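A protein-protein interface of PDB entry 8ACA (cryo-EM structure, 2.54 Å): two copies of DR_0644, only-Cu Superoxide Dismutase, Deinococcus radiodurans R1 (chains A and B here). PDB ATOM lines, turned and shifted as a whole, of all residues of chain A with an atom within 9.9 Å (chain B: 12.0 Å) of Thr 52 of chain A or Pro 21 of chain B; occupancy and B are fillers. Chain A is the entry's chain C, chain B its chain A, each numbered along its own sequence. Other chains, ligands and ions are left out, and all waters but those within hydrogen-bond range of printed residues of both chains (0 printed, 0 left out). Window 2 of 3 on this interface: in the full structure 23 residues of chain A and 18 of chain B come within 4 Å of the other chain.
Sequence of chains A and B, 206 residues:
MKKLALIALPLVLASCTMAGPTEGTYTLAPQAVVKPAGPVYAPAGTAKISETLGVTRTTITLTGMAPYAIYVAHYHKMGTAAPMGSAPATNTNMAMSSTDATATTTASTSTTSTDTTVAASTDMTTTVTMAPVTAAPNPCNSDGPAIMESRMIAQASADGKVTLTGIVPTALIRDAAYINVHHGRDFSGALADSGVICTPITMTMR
The backbone NH (N) of Gly 20 of chain B lies within hydrogen-bond range of the backbone carbonyl oxygen (O) of Glu 51 of chain A, at 3.1 Å.
The backbone carbonyl oxygen (O) of Thr 22 of chain B sits at hydrogen-bond distance from the backbone NH (N) of Glu 51 of chain A, at 2.8 Å.
N of Gly 24 of chain B lies within hydrogen-bond range of O of Ile 49 of chain A (3.4 Å).
The backbone carbonyl oxygen (O) of Ile 49 of chain A lies close to the backbone carbonyl oxygen (O) of Glu 23 of chain B (3.1 Å).
The backbone nitrogen (N) of Pro 21 of chain B sits close to the backbone carbonyl oxygen (O) of Glu 51 of chain A (3.2 Å).
The backbone NH (N) of Gly 20 of chain B sits at hydrogen-bond distance from the side-chain carboxylate (OE1) of Glu 23 of chain B.
N of Arg 57 of chain A sits at hydrogen-bond distance from O of Ser 50 of chain A, 3.1 Å away.
The side-chain carboxylate of Glu 51 of chain A lies within hydrogen-bond range of the backbone NH of Gly 54 of chain A, at 2.8 Å.
Among the printed residues, merely in contact across the chains: Thr 52 of chain A with Pro 21 of chain B (3.1 Å), Ser 50 of chain A with Glu 23 of chain B (3.4 Å), Ser 50 of chain A with Thr 22 of chain B (3.4 Å), Thr 52 of chain A with Gly 20 of chain B (3.7 Å) and Ser 50 of chain A with Gly 20 of chain B (3.9 Å).
Pro 21 of chain B touches just these residues of chain A: Glu 51 (3.2 Å) and Thr 52 (3.1 Å).
No residue of chain B comes within 4 Å of Gly 54 of chain A.
No residue of chain B comes within 4 Å of Val 55 of chain A.
No residue of chain B comes within 4 Å of Thr 56 of chain A.
Of the printed residues of chain A, Glu 23 of chain B touches Ile 49 and Ser 50.
Printed residues of chain B within 4 Å of Ile 49 of chain A: Glu 23 and Gly 24.
Ile 173 of chain A touches none of the printed residues of chain B.
Val 168 of chain A touches none of the printed residues of chain B.
The nearest residue of chain B that does not touch Thr 52 of chain A is Thr 22 of chain B (5.1 Å).
The nearest residue of chain A that does not touch Pro 21 of chain B is Leu 53 of chain A (4.8 Å).
Of the 16 printed residues of chain A, 4 touch a printed residue of chain B.
Printed residues of chain A that touch a printed residue of chain B: Ile 49, Ser 50, Glu 51 and Thr 52.
Of the 6 printed residues of chain B, 5 touch a printed residue of chain A.
Hydrophobic or aromatic side chains of chain B that line the printed part of chain A: Pro 21.
No position is printed for both chains.
Of the 10 pairs that touch across the chains among the printed residues, none has its exchanged pair printed and touching as well.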
ATOM      1  N   ILE A  49      34.030 -11.612  31.373  1.00  0.00           N
ATOM      2  CA  ILE A  49      33.459 -11.728  29.994  1.00  0.00           C
ATOM      3  C   ILE A  49      32.645 -13.015  29.870  1.00  0.00           C
ATOM      4  O   ILE A  49      33.225 -14.090  30.018  1.00  0.00           O
ATOM      5  CB  ILE A  49      34.548 -11.662  28.906  1.00  0.00           C
ATOM      6  CG1 ILE A  49      33.993 -12.055  27.537  1.00  0.00           C
ATOM      7  CG2 ILE A  49      35.755 -12.500  29.292  1.00  0.00           C
ATOM      8  CD1 ILE A  49      34.923 -11.753  26.392  1.00  0.00           C
ATOM      9  N   SER A  50      31.350 -12.897  29.585  1.00  0.00           N
ATOM     10  CA  SER A  50      30.459 -14.085  29.678  1.00  0.00           C
ATOM     11  C   SER A  50      29.726 -14.277  28.356  1.00  0.00           C
ATOM     12  O   SER A  50      28.982 -13.366  27.954  1.00  0.00           O
ATOM     13  CB  SER A  50      29.475 -13.926  30.797  1.00  0.00           C
ATOM     14  OG  SER A  50      28.600 -12.835  30.552  1.00  0.00           O
ATOM     15  N   GLU A  51      29.974 -15.400  27.672  1.00  0.00           N
ATOM     16  CA  GLU A  51      29.346 -15.655  26.344  1.00  0.00           C
ATOM     17  C   GLU A  51      28.088 -16.505  26.547  1.00  0.00           C
ATOM     18  O   GLU A  51      28.092 -17.342  27.472  1.00  0.00           O
ATOM     19  CB  GLU A  51      30.341 -16.364  25.422  1.00  0.00           C
ATOM     20  CG  GLU A  51      30.043 -16.176  23.946  1.00  0.00           C
ATOM     21  CD  GLU A  51      29.193 -17.272  23.326  1.00  0.00           C
ATOM     22  OE1 GLU A  51      29.448 -18.456  23.623  1.00  0.00           O
ATOM     23  OE2 GLU A  51      28.275 -16.937  22.555  1.00  0.00           O
ATOM     24  N   THR A  52      27.059 -16.210  25.753  1.00  0.00           N
ATOM     25  CA  THR A  52      25.794 -16.967  25.863  1.00  0.00           C
ATOM     26  C   THR A  52      25.456 -17.598  24.512  1.00  0.00           C
ATOM     27  O   THR A  52      26.044 -18.648  24.186  1.00  0.00           O
ATOM     28  CB  THR A  52      24.711 -16.154  26.597  1.00  0.00           C
ATOM     29  OG1 THR A  52      23.550 -16.931  26.898  1.00  0.00           O
ATOM     30  CG2 THR A  52      24.329 -14.877  25.881  1.00  0.00           C
ATOM     31  N   LEU A  53      24.572 -16.973  23.759  1.00  0.00           N
ATOM     32  CA  LEU A  53      24.100 -17.450  22.433  1.00  0.00           C
ATOM     33  C   LEU A  53      24.541 -16.450  21.361  1.00  0.00           C
ATOM     34  O   LEU A  53      23.660 -15.896  20.675  1.00  0.00           O
ATOM     35  CB  LEU A  53      22.574 -17.580  22.468  1.00  0.00           C
ATOM     36  CG  LEU A  53      22.037 -18.795  23.222  1.00  0.00           C
ATOM     37  CD1 LEU A  53      20.517 -18.807  23.217  1.00  0.00           C
ATOM     38  CD2 LEU A  53      22.584 -20.084  22.631  1.00  0.00           C
ATOM     39  N   GLY A  54      25.854 -16.232  21.231  1.00  0.00           N
ATOM     40  CA  GLY A  54      26.361 -15.313  20.192  1.00  0.00           C
ATOM     41  C   GLY A  54      26.485 -13.879  20.670  1.00  0.00           C
ATOM     42  O   GLY A  54      26.741 -13.011  19.824  1.00  0.00           O
ATOM     43  N   VAL A  55      26.325 -13.633  21.973  1.00  0.00           N
ATOM     44  CA  VAL A  55      26.511 -12.253  22.513  1.00  0.00           C
ATOM     45  C   VAL A  55      27.479 -12.304  23.689  1.00  0.00           C
ATOM     46  O   VAL A  55      27.554 -13.359  24.346  1.00  0.00           O
ATOM     47  CB  VAL A  55      25.174 -11.576  22.860  1.00  0.00           C
ATOM     48  CG1 VAL A  55      24.279 -11.346  21.652  1.00  0.00           C
ATOM     49  CG2 VAL A  55      24.440 -12.317  23.964  1.00  0.00           C
ATOM     50  N   THR A  56      28.217 -11.217  23.941  1.00  0.00           N
ATOM     51  CA  THR A  56      29.195 -11.195  25.065  1.00  0.00           C
ATOM     52  C   THR A  56      28.868 -10.054  26.034  1.00  0.00           C
ATOM     53  O   THR A  56      28.724  -8.909  25.565  1.00  0.00           O
ATOM     54  CB  THR A  56      30.650 -11.136  24.578  1.00  0.00           C
ATOM     55  OG1 THR A  56      30.823  -9.994  23.737  1.00  0.00           O
ATOM     56  CG2 THR A  56      31.079 -12.391  23.851  1.00  0.00           C
ATOM     57  N   ARG A  57      28.759 -10.365  27.330  1.00  0.00           N
ATOM     58  CA  ARG A  57      28.491  -9.321  28.355  1.00  0.00           C
ATOM     59  C   ARG A  57      29.729  -9.175  29.245  1.00  0.00           C
ATOM     60  O   ARG A  57      30.030 -10.125  29.994  1.00  0.00           O
ATOM     61  CB  ARG A  57      27.257  -9.687  29.185  1.00  0.00           C
ATOM     62  CG  ARG A  57      25.955  -9.666  28.399  1.00  0.00           C
ATOM     63  CD  ARG A  57      24.760  -9.987  29.276  1.00  0.00           C
ATOM     64  NE  ARG A  57      23.517 -10.039  28.522  1.00  0.00           N
ATOM     65  CZ  ARG A  57      22.347 -10.411  29.029  1.00  0.00           C
ATOM     66  NH1 ARG A  57      22.260 -10.769  30.298  1.00  0.00           N
ATOM     67  NH2 ARG A  57      21.270 -10.429  28.264  1.00  0.00           N
ATOM     68  N   THR A  58      30.386  -8.022  29.202  1.00  0.00           N
ATOM     69  CA  THR A  58      31.659  -7.760  29.926  1.00  0.00           C
ATOM     70  C   THR A  58      31.432  -6.834  31.126  1.00  0.00           C
ATOM     71  O   THR A  58      30.877  -5.750  30.924  1.00  0.00           O
ATOM     72  CB  THR A  58      32.682  -7.118  28.982  1.00  0.00           C
ATOM     73  OG1 THR A  58      32.114  -5.903  28.498  1.00  0.00           O
ATOM     74  CG2 THR A  58      33.052  -8.007  27.818  1.00  0.00           C
ATOM     75  N   GLY A 166      28.899  -3.881  29.011  1.00  0.00           N
ATOM     76  CA  GLY A 166      28.725  -3.720  27.551  1.00  0.00           C
ATOM     77  C   GLY A 166      28.230  -4.978  26.854  1.00  0.00           C
ATOM     78  O   GLY A 166      28.561  -6.072  27.333  1.00  0.00           O
ATOM     79  N   ILE A 167      27.447  -4.829  25.779  1.00  0.00           N
ATOM     80  CA  ILE A 167      26.935  -5.999  25.003  1.00  0.00           C
ATOM     81  C   ILE A 167      27.544  -5.943  23.596  1.00  0.00           C
ATOM     82  O   ILE A 167      27.337  -4.923  22.902  1.00  0.00           O
ATOM     83  CB  ILE A 167      25.390  -6.020  25.000  1.00  0.00           C
ATOM     84  CG1 ILE A 167      24.812  -7.277  24.343  1.00  0.00           C
ATOM     85  CG2 ILE A 167      24.829  -4.749  24.379  1.00  0.00           C
ATOM     86  CD1 ILE A 167      23.335  -7.476  24.598  1.00  0.00           C
ATOM     87  N   VAL A 168      28.305  -6.977  23.210  1.00  0.00           N
ATOM     88  CA  VAL A 168      29.013  -6.966  21.894  1.00  0.00           C
ATOM     89  C   VAL A 168      28.810  -8.311  21.181  1.00  0.00           C
ATOM     90  O   VAL A 168      29.007  -9.340  21.851  1.00  0.00           O
ATOM     91  CB  VAL A 168      30.522  -6.706  22.074  1.00  0.00           C
ATOM     92  CG1 VAL A 168      31.188  -6.281  20.776  1.00  0.00           C
ATOM     93  CG2 VAL A 168      30.825  -5.721  23.193  1.00  0.00           C
ATOM     94  N   PRO A 169      28.425  -8.383  19.889  1.00  0.00           N
ATOM     95  CA  PRO A 169      28.353  -9.676  19.206  1.00  0.00           C
ATOM     96  C   PRO A 169      29.713 -10.389  19.275  1.00  0.00           C
ATOM     97  O   PRO A 169      30.716  -9.714  19.178  1.00  0.00           O
ATOM     98  CB  PRO A 169      28.009  -9.274  17.770  1.00  0.00           C
ATOM     99  CG  PRO A 169      27.271  -7.967  17.919  1.00  0.00           C
ATOM    100  CD  PRO A 169      27.999  -7.265  19.043  1.00  0.00           C
ATOM    101  N   THR A 170      29.724 -11.715  19.429  1.00  0.00           N
ATOM    102  CA  THR A 170      30.984 -12.497  19.546  1.00  0.00           C
ATOM    103  C   THR A 170      31.804 -12.362  18.256  1.00  0.00           C
ATOM    104  O   THR A 170      33.039 -12.219  18.359  1.00  0.00           O
ATOM    105  CB  THR A 170      30.689 -13.956  19.917  1.00  0.00           C
ATOM    106  OG1 THR A 170      29.778 -13.942  21.016  1.00  0.00           O
ATOM    107  CG2 THR A 170      31.930 -14.735  20.297  1.00  0.00           C
ATOM    108  N   ILE A 173      33.903  -9.252  18.409  1.00  0.00           N
ATOM    109  CA  ILE A 173      35.106  -9.350  19.294  1.00  0.00           C
ATOM    110  C   ILE A 173      36.009 -10.525  18.905  1.00  0.00           C
ATOM    111  O   ILE A 173      36.953 -10.800  19.672  1.00  0.00           O
ATOM    112  CB  ILE A 173      34.721  -9.374  20.787  1.00  0.00           C
ATOM    113  CG1 ILE A 173      33.675 -10.445  21.104  1.00  0.00           C
ATOM    114  CG2 ILE A 173      34.275  -7.996  21.246  1.00  0.00           C
ATOM    115  CD1 ILE A 173      34.196 -11.572  21.965  1.00  0.00           C
ATOM    116  N   GLY B  20      26.754 -16.615  30.131  1.00  0.00           N
ATOM    117  CA  GLY B  20      25.911 -17.766  29.755  1.00  0.00           C
ATOM    118  C   GLY B  20      26.700 -19.061  29.768  1.00  0.00           C
ATOM    119  O   GLY B  20      27.400 -19.309  30.771  1.00  0.00           O
ATOM    120  N   PRO B  21      26.641 -19.903  28.712  1.00  0.00           N
ATOM    121  CA  PRO B  21      27.328 -21.207  28.697  1.00  0.00           C
ATOM    122  C   PRO B  21      28.833 -21.046  28.950  1.00  0.00           C
ATOM    123  O   PRO B  21      29.432 -21.954  29.496  1.00  0.00           O
ATOM    124  CB  PRO B  21      27.114 -21.759  27.281  1.00  0.00           C
ATOM    125  CG  PRO B  21      25.853 -21.082  26.816  1.00  0.00           C
ATOM    126  CD  PRO B  21      25.951 -19.694  27.410  1.00  0.00           C
ATOM    127  N   THR B  22      29.396 -19.902  28.554  1.00  0.00           N
ATOM    128  CA  THR B  22      30.853 -19.661  28.731  1.00  0.00           C
ATOM    129  C   THR B  22      31.063 -18.464  29.661  1.00  0.00           C
ATOM    130  O   THR B  22      30.340 -17.462  29.496  1.00  0.00           O
ATOM    131  CB  THR B  22      31.535 -19.432  27.377  1.00  0.00           C
ATOM    132  OG1 THR B  22      31.351 -20.613  26.596  1.00  0.00           O
ATOM    133  CG2 THR B  22      33.011 -19.128  27.508  1.00  0.00           C
ATOM    134  N   GLU B  23      32.007 -18.572  30.603  1.00  0.00           N
ATOM    135  CA  GLU B  23      32.322 -17.446  31.519  1.00  0.00           C
ATOM    136  C   GLU B  23      33.745 -16.932  31.268  1.00  0.00           C
ATOM    137  O   GLU B  23      34.225 -17.066  30.133  1.00  0.00           O
ATOM    138  CB  GLU B  23      32.083 -17.876  32.964  1.00  0.00           C
ATOM    139  CG  GLU B  23      30.707 -18.471  33.207  1.00  0.00           C
ATOM    140  CD  GLU B  23      29.612 -17.473  33.546  1.00  0.00           C
ATOM    141  OE1 GLU B  23      29.176 -16.742  32.641  1.00  0.00           O
ATOM    142  OE2 GLU B  23      29.193 -17.439  34.716  1.00  0.00           O
ATOM    143  N   GLY B  24      34.377 -16.355  32.298  1.00  0.00           N
ATOM    144  CA  GLY B  24      35.734 -15.779  32.199  1.00  0.00           C
ATOM    145  C   GLY B  24      35.916 -14.749  33.303  1.00  0.00           C
ATOM    146  O   GLY B  24      34.936 -14.068  33.587  1.00  0.00           O
ATOM    147  N   THR B  25      37.097 -14.701  33.932  1.00  0.00           N
ATOM    148  CA  THR B  25      37.392 -13.731  35.024  1.00  0.00           C
ATOM    149  C   THR B  25      38.857 -13.306  34.894  1.00  0.00           C
ATOM    150  O   THR B  25      39.723 -14.206  34.910  1.00  0.00           O
ATOM    151  CB  THR B  25      37.106 -14.340  36.403  1.00  0.00           C
ATOM    152  OG1 THR B  25      35.711 -14.635  36.490  1.00  0.00           O
ATOM    153  CG2 THR B  25      37.501 -13.428  37.545  1.00  0.00           C
